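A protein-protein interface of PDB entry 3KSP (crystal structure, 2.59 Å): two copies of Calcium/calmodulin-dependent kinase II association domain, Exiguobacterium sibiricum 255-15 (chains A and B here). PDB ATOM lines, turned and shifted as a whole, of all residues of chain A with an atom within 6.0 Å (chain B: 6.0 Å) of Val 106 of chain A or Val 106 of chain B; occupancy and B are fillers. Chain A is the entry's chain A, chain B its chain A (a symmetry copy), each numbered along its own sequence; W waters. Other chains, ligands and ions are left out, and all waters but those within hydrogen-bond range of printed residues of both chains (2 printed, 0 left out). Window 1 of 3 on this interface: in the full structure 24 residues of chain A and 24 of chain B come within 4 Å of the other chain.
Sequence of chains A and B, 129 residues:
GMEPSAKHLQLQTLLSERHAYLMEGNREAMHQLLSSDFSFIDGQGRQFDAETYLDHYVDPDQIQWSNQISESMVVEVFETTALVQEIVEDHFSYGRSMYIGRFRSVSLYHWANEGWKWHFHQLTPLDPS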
ATOM      1  N   LEU A  83      17.553  13.954  -5.653  1.00  0.00           N
ATOM      2  CA  LEU A  83      17.993  12.644  -6.155  1.00  0.00           C
ATOM      3  C   LEU A  83      18.310  12.807  -7.646  1.00  0.00           C
ATOM      4  O   LEU A  83      17.433  13.219  -8.437  1.00  0.00           O
ATOM      5  CB  LEU A  83      16.900  11.589  -5.954  1.00  0.00           C
ATOM      6  CG  LEU A  83      17.254  10.150  -6.367  1.00  0.00           C
ATOM      7  CD1 LEU A  83      18.019   9.408  -5.257  1.00  0.00           C
ATOM      8  CD2 LEU A  83      15.986   9.389  -6.750  1.00  0.00           C
ATOM      9  N   VAL A  84      19.554  12.500  -8.013  1.00  0.00           N
ATOM     10  CA  VAL A  84      20.025  12.647  -9.380  1.00  0.00           C
ATOM     11  C   VAL A  84      20.392  11.278  -9.964  1.00  0.00           C
ATOM     12  O   VAL A  84      21.109  10.506  -9.335  1.00  0.00           O
ATOM     13  CB  VAL A  84      21.238  13.591  -9.424  1.00  0.00           C
ATOM     14  CG1 VAL A  84      21.779  13.705 -10.844  1.00  0.00           C
ATOM     15  CG2 VAL A  84      20.852  14.971  -8.834  1.00  0.00           C
ATOM     16  N   GLN A  85      19.862  10.970 -11.142  1.00  0.00           N
ATOM     17  CA  GLN A  85      20.216   9.737 -11.868  1.00  0.00           C
ATOM     18  C   GLN A  85      20.941  10.139 -13.148  1.00  0.00           C
ATOM     19  O   GLN A  85      20.514  11.042 -13.861  1.00  0.00           O
ATOM     20  CB  GLN A  85      18.987   8.886 -12.217  1.00  0.00           C
ATOM     21  CG  GLN A  85      18.134   8.547 -11.025  1.00  0.00           C
ATOM     22  CD  GLN A  85      16.770   8.029 -11.412  1.00  0.00           C
ATOM     23  OE1 GLN A  85      16.646   7.083 -12.185  1.00  0.00           O
ATOM     24  NE2 GLN A  85      15.739   8.638 -10.865  1.00  0.00           N
ATOM     25  N   GLU A  86      22.035   9.465 -13.437  1.00  0.00           N
ATOM     26  CA  GLU A  86      22.866   9.851 -14.546  1.00  0.00           C
ATOM     27  C   GLU A  86      23.487   8.625 -15.199  1.00  0.00           C
ATOM     28  O   GLU A  86      23.789   7.660 -14.515  1.00  0.00           O
ATOM     29  CB  GLU A  86      23.949  10.783 -14.032  1.00  0.00           C
ATOM     30  CG  GLU A  86      24.594  11.592 -15.122  1.00  0.00           C
ATOM     31  CD  GLU A  86      25.612  12.600 -14.598  1.00  0.00           C
ATOM     32  OE1 GLU A  86      25.924  12.538 -13.377  1.00  0.00           O
ATOM     33  OE2 GLU A  86      26.073  13.437 -15.418  1.00  0.00           O
ATOM     34  N   ARG A 104      25.754   3.574 -14.661  1.00  0.00           N
ATOM     35  CA  ARG A 104      24.489   4.152 -14.253  1.00  0.00           C
ATOM     36  C   ARG A 104      24.728   4.585 -12.822  1.00  0.00           C
ATOM     37  O   ARG A 104      25.097   3.771 -11.979  1.00  0.00           O
ATOM     38  CB  ARG A 104      23.369   3.115 -14.350  1.00  0.00           C
ATOM     39  CG  ARG A 104      22.034   3.563 -13.815  1.00  0.00           C
ATOM     40  CD  ARG A 104      21.609   4.924 -14.343  1.00  0.00           C
ATOM     41  NE  ARG A 104      20.286   5.261 -13.825  1.00  0.00           N
ATOM     42  CZ  ARG A 104      19.169   5.227 -14.544  1.00  0.00           C
ATOM     43  NH1 ARG A 104      19.229   4.914 -15.831  1.00  0.00           N
ATOM     44  NH2 ARG A 104      18.003   5.518 -13.986  1.00  0.00           N
ATOM     45  N   SER A 105      24.564   5.872 -12.538  1.00  0.00           N
ATOM     46  CA  SER A 105      24.845   6.377 -11.193  1.00  0.00           C
ATOM     47  C   SER A 105      23.617   7.030 -10.561  1.00  0.00           C
ATOM     48  O   SER A 105      22.730   7.530 -11.282  1.00  0.00           O
ATOM     49  CB  SER A 105      26.001   7.368 -11.232  1.00  0.00           C
ATOM     50  OG  SER A 105      25.545   8.625 -11.654  1.00  0.00           O
ATOM     51  N   VAL A 106      23.555   6.965  -9.220  1.00  0.00           N
ATOM     52  CA  VAL A 106      22.569   7.685  -8.418  1.00  0.00           C
ATOM     53  C   VAL A 106      23.284   8.473  -7.338  1.00  0.00           C
ATOM     54  O   VAL A 106      24.258   8.009  -6.787  1.00  0.00           O
ATOM     55  CB  VAL A 106      21.497   6.775  -7.792  1.00  0.00           C
ATOM     56  CG1 VAL A 106      22.094   5.652  -6.924  1.00  0.00           C
ATOM     57  CG2 VAL A 106      20.479   7.644  -7.027  1.00  0.00           C
ATOM     58  N   SER A 107      22.812   9.690  -7.074  1.00  0.00           N
ATOM     59  CA  SER A 107      23.361  10.543  -6.020  1.00  0.00           C
ATOM     60  C   SER A 107      22.247  11.184  -5.234  1.00  0.00           C
ATOM     61  O   SER A 107      21.123  11.346  -5.721  1.00  0.00           O
ATOM     62  CB  SER A 107      24.192  11.649  -6.641  1.00  0.00           C
ATOM     63  OG  SER A 107      24.398  11.361  -8.000  1.00  0.00           O
ATOM     64  N   LEU A 108      22.567  11.543  -4.004  1.00  0.00           N
ATOM     65  CA  LEU A 108      21.664  12.315  -3.172  1.00  0.00           C
ATOM     66  C   LEU A 108      22.413  13.564  -2.690  1.00  0.00           C
ATOM     67  O   LEU A 108      23.585  13.487  -2.279  1.00  0.00           O
ATOM     68  CB  LEU A 108      21.186  11.499  -1.983  1.00  0.00           C
ATOM     69  CG  LEU A 108      19.955  12.062  -1.280  1.00  0.00           C
ATOM     70  CD1 LEU A 108      18.704  11.656  -2.037  1.00  0.00           C
ATOM     71  CD2 LEU A 108      19.868  11.572   0.138  1.00  0.00           C
ATOM     72  N   PHE A 120      25.645  11.360  -0.968  1.00  0.00           N
ATOM     73  CA  PHE A 120      25.771   9.942  -1.339  1.00  0.00           C
ATOM     74  C   PHE A 120      25.956   9.795  -2.846  1.00  0.00           C
ATOM     75  O   PHE A 120      25.394  10.589  -3.629  1.00  0.00           O
ATOM     76  CB  PHE A 120      24.500   9.193  -0.930  1.00  0.00           C
ATOM     77  CG  PHE A 120      24.523   7.760  -1.267  1.00  0.00           C
ATOM     78  CD1 PHE A 120      25.136   6.859  -0.430  1.00  0.00           C
ATOM     79  CD2 PHE A 120      23.965   7.310  -2.440  1.00  0.00           C
ATOM     80  CE1 PHE A 120      25.198   5.511  -0.759  1.00  0.00           C
ATOM     81  CE2 PHE A 120      23.994   5.963  -2.767  1.00  0.00           C
ATOM     82  CZ  PHE A 120      24.621   5.073  -1.930  1.00  0.00           C
ATOM     83  N   HIS A 121      26.732   8.787  -3.243  1.00  0.00           N
ATOM     84  CA  HIS A 121      26.865   8.429  -4.653  1.00  0.00           C
ATOM     85  C   HIS A 121      27.030   6.940  -4.778  1.00  0.00           C
ATOM     86  O   HIS A 121      27.656   6.346  -3.928  1.00  0.00           O
ATOM     87  CB  HIS A 121      28.072   9.129  -5.281  1.00  0.00           C
ATOM     88  CG  HIS A 121      28.009   9.244  -6.773  1.00  0.00           C
ATOM     89  ND1 HIS A 121      27.124  10.094  -7.419  1.00  0.00           N
ATOM     90  CD2 HIS A 121      28.758   8.670  -7.746  1.00  0.00           C
ATOM     91  CE1 HIS A 121      27.320  10.010  -8.728  1.00  0.00           C
ATOM     92  NE2 HIS A 121      28.308   9.160  -8.953  1.00  0.00           N
ATOM     93  N   GLN A 122      26.469   6.342  -5.833  1.00  0.00           N
ATOM     94  CA  GLN A 122      26.652   4.907  -6.092  1.00  0.00           C
ATOM     95  C   GLN A 122      26.698   4.645  -7.593  1.00  0.00           C
ATOM     96  O   GLN A 122      25.912   5.212  -8.362  1.00  0.00           O
ATOM     97  CB  GLN A 122      25.558   4.050  -5.405  1.00  0.00           C
ATOM     98  CG  GLN A 122      25.639   2.526  -5.672  1.00  0.00           C
ATOM     99  CD  GLN A 122      24.850   1.673  -4.677  1.00  0.00           C
ATOM    100  OE1 GLN A 122      24.650   2.058  -3.521  1.00  0.00           O
ATOM    101  NE2 GLN A 122      24.441   0.472  -5.116  1.00  0.00           N
ATOM    102  N   LEU A 123      27.639   3.785  -7.984  1.00  0.00           N
ATOM    103  CA  LEU A 123      27.848   3.375  -9.383  1.00  0.00           C
ATOM    104  C   LEU A 123      27.369   1.930  -9.659  1.00  0.00           C
ATOM    105  O   LEU A 123      27.590   1.021  -8.834  1.00  0.00           O
ATOM    106  CB  LEU A 123      29.352   3.428  -9.744  1.00  0.00           C
ATOM    107  CG  LEU A 123      30.041   4.783  -9.792  1.00  0.00           C
ATOM    108  CD1 LEU A 123      31.449   4.576 -10.460  1.00  0.00           C
ATOM    109  CD2 LEU A 123      29.144   5.884 -10.486  1.00  0.00           C
ATOM    110  N   LEU B  83      16.589   7.531   2.856  1.00  0.00           N
ATOM    111  CA  LEU B  83      17.613   6.870   2.036  1.00  0.00           C
ATOM    112  C   LEU B  83      18.092   5.634   2.807  1.00  0.00           C
ATOM    113  O   LEU B  83      18.574   5.755   3.956  1.00  0.00           O
ATOM    114  CB  LEU B  83      18.788   7.816   1.762  1.00  0.00           C
ATOM    115  CG  LEU B  83      19.901   7.277   0.849  1.00  0.00           C
ATOM    116  CD1 LEU B  83      19.556   7.453  -0.641  1.00  0.00           C
ATOM    117  CD2 LEU B  83      21.227   7.962   1.180  1.00  0.00           C
ATOM    118  N   VAL B  84      17.944   4.465   2.184  1.00  0.00           N
ATOM    119  CA  VAL B  84      18.304   3.199   2.802  1.00  0.00           C
ATOM    120  C   VAL B  84      19.446   2.536   2.022  1.00  0.00           C
ATOM    121  O   VAL B  84      19.383   2.426   0.802  1.00  0.00           O
ATOM    122  CB  VAL B  84      17.081   2.270   2.855  1.00  0.00           C
ATOM    123  CG1 VAL B  84      17.460   0.916   3.443  1.00  0.00           C
ATOM    124  CG2 VAL B  84      15.936   2.950   3.647  1.00  0.00           C
ATOM    125  N   GLN B  85      20.498   2.140   2.729  1.00  0.00           N
ATOM    126  CA  GLN B  85      21.616   1.392   2.126  1.00  0.00           C
ATOM    127  C   GLN B  85      21.629  -0.004   2.739  1.00  0.00           C
ATOM    128  O   GLN B  85      21.506  -0.166   3.949  1.00  0.00           O
ATOM    129  CB  GLN B  85      22.974   2.070   2.359  1.00  0.00           C
ATOM    130  CG  GLN B  85      23.015   3.502   1.900  1.00  0.00           C
ATOM    131  CD  GLN B  85      24.204   4.255   2.444  1.00  0.00           C
ATOM    132  OE1 GLN B  85      25.346   3.830   2.297  1.00  0.00           O
ATOM    133  NE2 GLN B  85      23.943   5.386   3.064  1.00  0.00           N
ATOM    134  N   GLU B  86      21.782  -1.010   1.901  1.00  0.00           N
ATOM    135  CA  GLU B  86      21.674  -2.370   2.357  1.00  0.00           C
ATOM    136  C   GLU B  86      22.630  -3.268   1.586  1.00  0.00           C
ATOM    137  O   GLU B  86      22.871  -3.032   0.412  1.00  0.00           O
ATOM    138  CB  GLU B  86      20.241  -2.829   2.159  1.00  0.00           C
ATOM    139  CG  GLU B  86      19.894  -4.040   2.981  1.00  0.00           C
ATOM    140  CD  GLU B  86      18.427  -4.444   2.861  1.00  0.00           C
ATOM    141  OE1 GLU B  86      17.726  -3.857   1.993  1.00  0.00           O
ATOM    142  OE2 GLU B  86      18.009  -5.336   3.644  1.00  0.00           O
ATOM    143  N   ARG B 104      25.094  -4.587  -3.224  1.00  0.00           N
ATOM    144  CA  ARG B 104      25.030  -3.375  -2.432  1.00  0.00           C
ATOM    145  C   ARG B 104      23.888  -2.593  -3.048  1.00  0.00           C
ATOM    146  O   ARG B 104      23.907  -2.302  -4.242  1.00  0.00           O
ATOM    147  CB  ARG B 104      26.350  -2.608  -2.516  1.00  0.00           C
ATOM    148  CG  ARG B 104      26.351  -1.258  -1.846  1.00  0.00           C
ATOM    149  CD  ARG B 104      25.795  -1.298  -0.432  1.00  0.00           C
ATOM    150  NE  ARG B 104      25.881   0.030   0.167  1.00  0.00           N
ATOM    151  CZ  ARG B 104      26.765   0.378   1.096  1.00  0.00           C
ATOM    152  NH1 ARG B 104      27.610  -0.529   1.565  1.00  0.00           N
ATOM    153  NH2 ARG B 104      26.794   1.617   1.565  1.00  0.00           N
ATOM    154  N   SER B 105      22.866  -2.282  -2.261  1.00  0.00           N
ATOM    155  CA  SER B 105      21.695  -1.589  -2.803  1.00  0.00           C
ATOM    156  C   SER B 105      21.447  -0.254  -2.101  1.00  0.00           C
ATOM    157  O   SER B 105      21.833  -0.080  -0.928  1.00  0.00           O
ATOM    158  CB  SER B 105      20.460  -2.474  -2.692  1.00  0.00           C
ATOM    159  OG  SER B 105      19.942  -2.419  -1.390  1.00  0.00           O
ATOM    160  N   VAL B 106      20.857   0.690  -2.852  1.00  0.00           N
ATOM    161  CA  VAL B 106      20.365   1.959  -2.320  1.00  0.00           C
ATOM    162  C   VAL B 106      18.922   2.152  -2.742  1.00  0.00           C
ATOM    163  O   VAL B 106      18.555   1.799  -3.842  1.00  0.00           O
ATOM    164  CB  VAL B 106      21.211   3.175  -2.741  1.00  0.00           C
ATOM    165  CG1 VAL B 106      21.344   3.315  -4.269  1.00  0.00           C
ATOM    166  CG2 VAL B 106      20.642   4.442  -2.073  1.00  0.00           C
ATOM    167  N   SER B 107      18.100   2.678  -1.838  1.00  0.00           N
ATOM    168  CA  SER B 107      16.695   2.978  -2.119  1.00  0.00           C
ATOM    169  C   SER B 107      16.328   4.330  -1.567  1.00  0.00           C
ATOM    170  O   SER B 107      16.956   4.839  -0.631  1.00  0.00           O
ATOM    171  CB  SER B 107      15.810   1.944  -1.449  1.00  0.00           C
ATOM    172  OG  SER B 107      16.608   0.880  -0.997  1.00  0.00           O
ATOM    173  N   LEU B 108      15.306   4.917  -2.163  1.00  0.00           N
ATOM    174  CA  LEU B 108      14.725   6.144  -1.654  1.00  0.00           C
ATOM    175  C   LEU B 108      13.222   5.911  -1.455  1.00  0.00           C
ATOM    176  O   LEU B 108      12.549   5.317  -2.316  1.00  0.00           O
ATOM    177  CB  LEU B 108      14.953   7.297  -2.618  1.00  0.00           C
ATOM    178  CG  LEU B 108      14.738   8.680  -2.015  1.00  0.00           C
ATOM    179  CD1 LEU B 108      15.979   9.102  -1.247  1.00  0.00           C
ATOM    180  CD2 LEU B 108      14.435   9.696  -3.081  1.00  0.00           C
ATOM    181  N   PHE B 120      12.550   4.668  -5.489  1.00  0.00           N
ATOM    182  CA  PHE B 120      13.729   4.327  -6.298  1.00  0.00           C
ATOM    183  C   PHE B 120      14.506   3.179  -5.659  1.00  0.00           C
ATOM    184  O   PHE B 120      14.558   3.071  -4.415  1.00  0.00           O
ATOM    185  CB  PHE B 120      14.652   5.545  -6.392  1.00  0.00           C
ATOM    186  CG  PHE B 120      15.874   5.302  -7.179  1.00  0.00           C
ATOM    187  CD1 PHE B 120      15.851   5.408  -8.549  1.00  0.00           C
ATOM    188  CD2 PHE B 120      17.042   4.931  -6.557  1.00  0.00           C
ATOM    189  CE1 PHE B 120      16.986   5.143  -9.302  1.00  0.00           C
ATOM    190  CE2 PHE B 120      18.191   4.690  -7.295  1.00  0.00           C
ATOM    191  CZ  PHE B 120      18.153   4.786  -8.664  1.00  0.00           C
ATOM    192  N   HIS B 121      15.103   2.338  -6.503  1.00  0.00           N
ATOM    193  CA  HIS B 121      16.011   1.294  -6.033  1.00  0.00           C
ATOM    194  C   HIS B 121      17.104   1.089  -7.043  1.00  0.00           C
ATOM    195  O   HIS B 121      16.840   1.194  -8.222  1.00  0.00           O
ATOM    196  CB  HIS B 121      15.262  -0.023  -5.818  1.00  0.00           C
ATOM    197  CG  HIS B 121      15.947  -0.976  -4.888  1.00  0.00           C
ATOM    198  ND1 HIS B 121      16.036  -0.753  -3.523  1.00  0.00           N
ATOM    199  CD2 HIS B 121      16.522  -2.184  -5.111  1.00  0.00           C
ATOM    200  CE1 HIS B 121      16.661  -1.776  -2.956  1.00  0.00           C
ATOM    201  NE2 HIS B 121      16.960  -2.659  -3.894  1.00  0.00           N
ATOM    202  N   GLN B 122      18.325   0.798  -6.585  1.00  0.00           N
ATOM    203  CA  GLN B 122      19.436   0.490  -7.494  1.00  0.00           C
ATOM    204  C   GLN B 122      20.357  -0.550  -6.867  1.00  0.00           C
ATOM    205  O   GLN B 122      20.672  -0.483  -5.673  1.00  0.00           O
ATOM    206  CB  GLN B 122      20.221   1.763  -7.903  1.00  0.00           C
ATOM    207  CG  GLN B 122      21.449   1.524  -8.818  1.00  0.00           C
ATOM    208  CD  GLN B 122      21.941   2.777  -9.545  1.00  0.00           C
ATOM    209  OE1 GLN B 122      21.170   3.701  -9.823  1.00  0.00           O
ATOM    210  NE2 GLN B 122      23.234   2.788  -9.905  1.00  0.00           N
ATOM    211  N   LEU B 123      20.767  -1.509  -7.697  1.00  0.00           N
ATOM    212  CA  LEU B 123      21.675  -2.602  -7.306  1.00  0.00           C
ATOM    213  C   LEU B 123      23.098  -2.431  -7.884  1.00  0.00           C
ATOM    214  O   LEU B 123      23.263  -2.042  -9.057  1.00  0.00           O
ATOM    215  CB  LEU B 123      21.140  -3.960  -7.820  1.00  0.00           C
ATOM    216  CG  LEU B 123      19.849  -4.505  -7.228  1.00  0.00           C
ATOM    217  CD1 LEU B 123      19.703  -5.997  -7.700  1.00  0.00           C
ATOM    218  CD2 LEU B 123      19.779  -4.305  -5.662  1.00  0.00           C
HETATM  219  O   HOH W   1      20.471   5.825 -11.362  1.00  0.00           O
HETATM  220  O   HOH W   2      24.154   1.544  -0.902  1.00  0.00           O
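Water W1 lies within hydrogen-bond range of NE of Arg 104 of chain A (2.5 Å), OE1 of Gln 122 of chain B (2.7 Å) and O of Ser 105 of chain A (2.8 Å).
Water W2 lies within hydrogen-bond range of NE of Arg 104 of chain B (2.5 Å), OE1 of Gln 122 of chain A (2.7 Å) and O of Ser 105 of chain B (2.8 Å).
The side-chain amide oxygen (OE1) of Gln 85 of chain A sits at hydrogen-bond distance from the guanidinium group (NH2) of Arg 104 of chain A (2.7 Å).
N of Gln 122 of chain A lies within hydrogen-bond range of O of Val 106 of chain A (2.9 Å).
The backbone NH of Leu 108 of chain A lies within hydrogen-bond range of the backbone carbonyl oxygen of Phe 120 of chain A (3.0 Å).
OE1 of Gln 85 of chain B sits at hydrogen-bond distance from NH2 of Arg 104 of chain B (2.7 Å).
The backbone NH of Gln 122 of chain B lies within hydrogen-bond range of the backbone carbonyl oxygen of Val 106 of chain B (2.9 Å).
The backbone NH (N) of Leu 108 of chain B lies within hydrogen-bond range of the backbone carbonyl oxygen (O) of Phe 120 of chain B.
Of chain B, only Val 106, Phe 120 and Gln 122 come within 4 Å of Val 106 of chain A.
Of chain A, only Val 106, Phe 120 and Gln 122 come within 4 Å of Val 106 of chain B.
Printed residues of chain B within 4 Å of Leu 83 of chain A: Leu 108 (3.995 Å).
Of the printed residues of chain A, Phe 120 of chain B touches Gln 85 and Val 106.
Of the printed residues of chain B, Gln 85 of chain A touches Phe 120.
Of the printed residues of chain A, Arg 104 of chain B touches Gln 122.
Of the printed residues of chain B, Gln 122 of chain A touches Arg 104, Val 106 and Gln 122.
His 121 of chain A touches none of the printed residues of chain B.
The nearest printed residue of chain A that does not touch Val 106 of chain B is Leu 83 of chain A (6.5 Å).
The nearest printed residue of chain B that does not touch Leu 108 of chain A is Val 106 of chain B (7.1 Å).
CD2 of Leu 108 of chain B touches CD2 of Leu 83 of chain A, 3.995 Å away.
OE1 of Gln 85 of chain A touches CE1 of Phe 120 of chain B, at 3.5 Å.
Val 106 of chain A touches Val 106 of chain B (CG1 to CG1, 3.6 Å).
Val 106 of chain A touches Phe 120 of chain B.
Val 106 of chain A touches Gln 122 of chain B (CG1 to OE1, 3.6 Å).
Leu 108 of chain A touches Leu 83 of chain B (CD2 to CD2, 3.996 Å).
Gln 85 of chain B touches Phe 120 of chain A.
Phe 120 of chain A touches Val 106 of chain B.
Gln 122 of chain A touches Val 106 of chain B.
Gln 122 of chain B touches Gln 122 of chain A.
The backbone carbonyl oxygen of Arg 104 of chain A lies within hydrogen-bond range of the side-chain amide nitrogen of Gln 122 of chain B, 3.0 Å away.
The side-chain amide nitrogen (NE2) of Gln 122 of chain A sits at hydrogen-bond distance from the backbone carbonyl oxygen (O) of Arg 104 of chain B, at 3.0 Å.
Of the 13 printed residues of chain B, 7 touch a printed residue of chain A.
Printed residues of chain B that touch a printed residue of chain A: Leu 83, Gln 85, Arg 104, Val 106, Leu 108, Phe 120 and Gln 122.
Hydrophobic or aromatic side chains of chain B within 4 Å of the printed part of chain A: Leu 83, Val 106, Leu 108 and Phe 120.
Hydrophobic or aromatic side chains of chain A within 4 Å of the printed part of chain B: Leu 83, Val 106, Leu 108 and Phe 120.
Arg 104 of chain A touches Gln 122 of chain B, and with the chains exchanged Gln 122 of chain A touches Arg 104 of chain B.
Val 106 of chain A touches Phe 120 of chain B, and with the chains exchanged Phe 120 of chain A touches Val 106 of chain B.
Val 106 of chain A touches Gln 122 of chain B, and with the chains exchanged Gln 122 of chain A touches Val 106 of chain B.
Gln 122 of chain B touches its own counterpart, Gln 122 of chain A.
Positions printed for both chains: 83, 84, 85, 86, 104, 105, 106, 107, 108, 120, 121, 122 and 123.
Of the 13 pairs that touch across the chains among the printed residues, 13 have their exchanged pair printed and touching as well.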
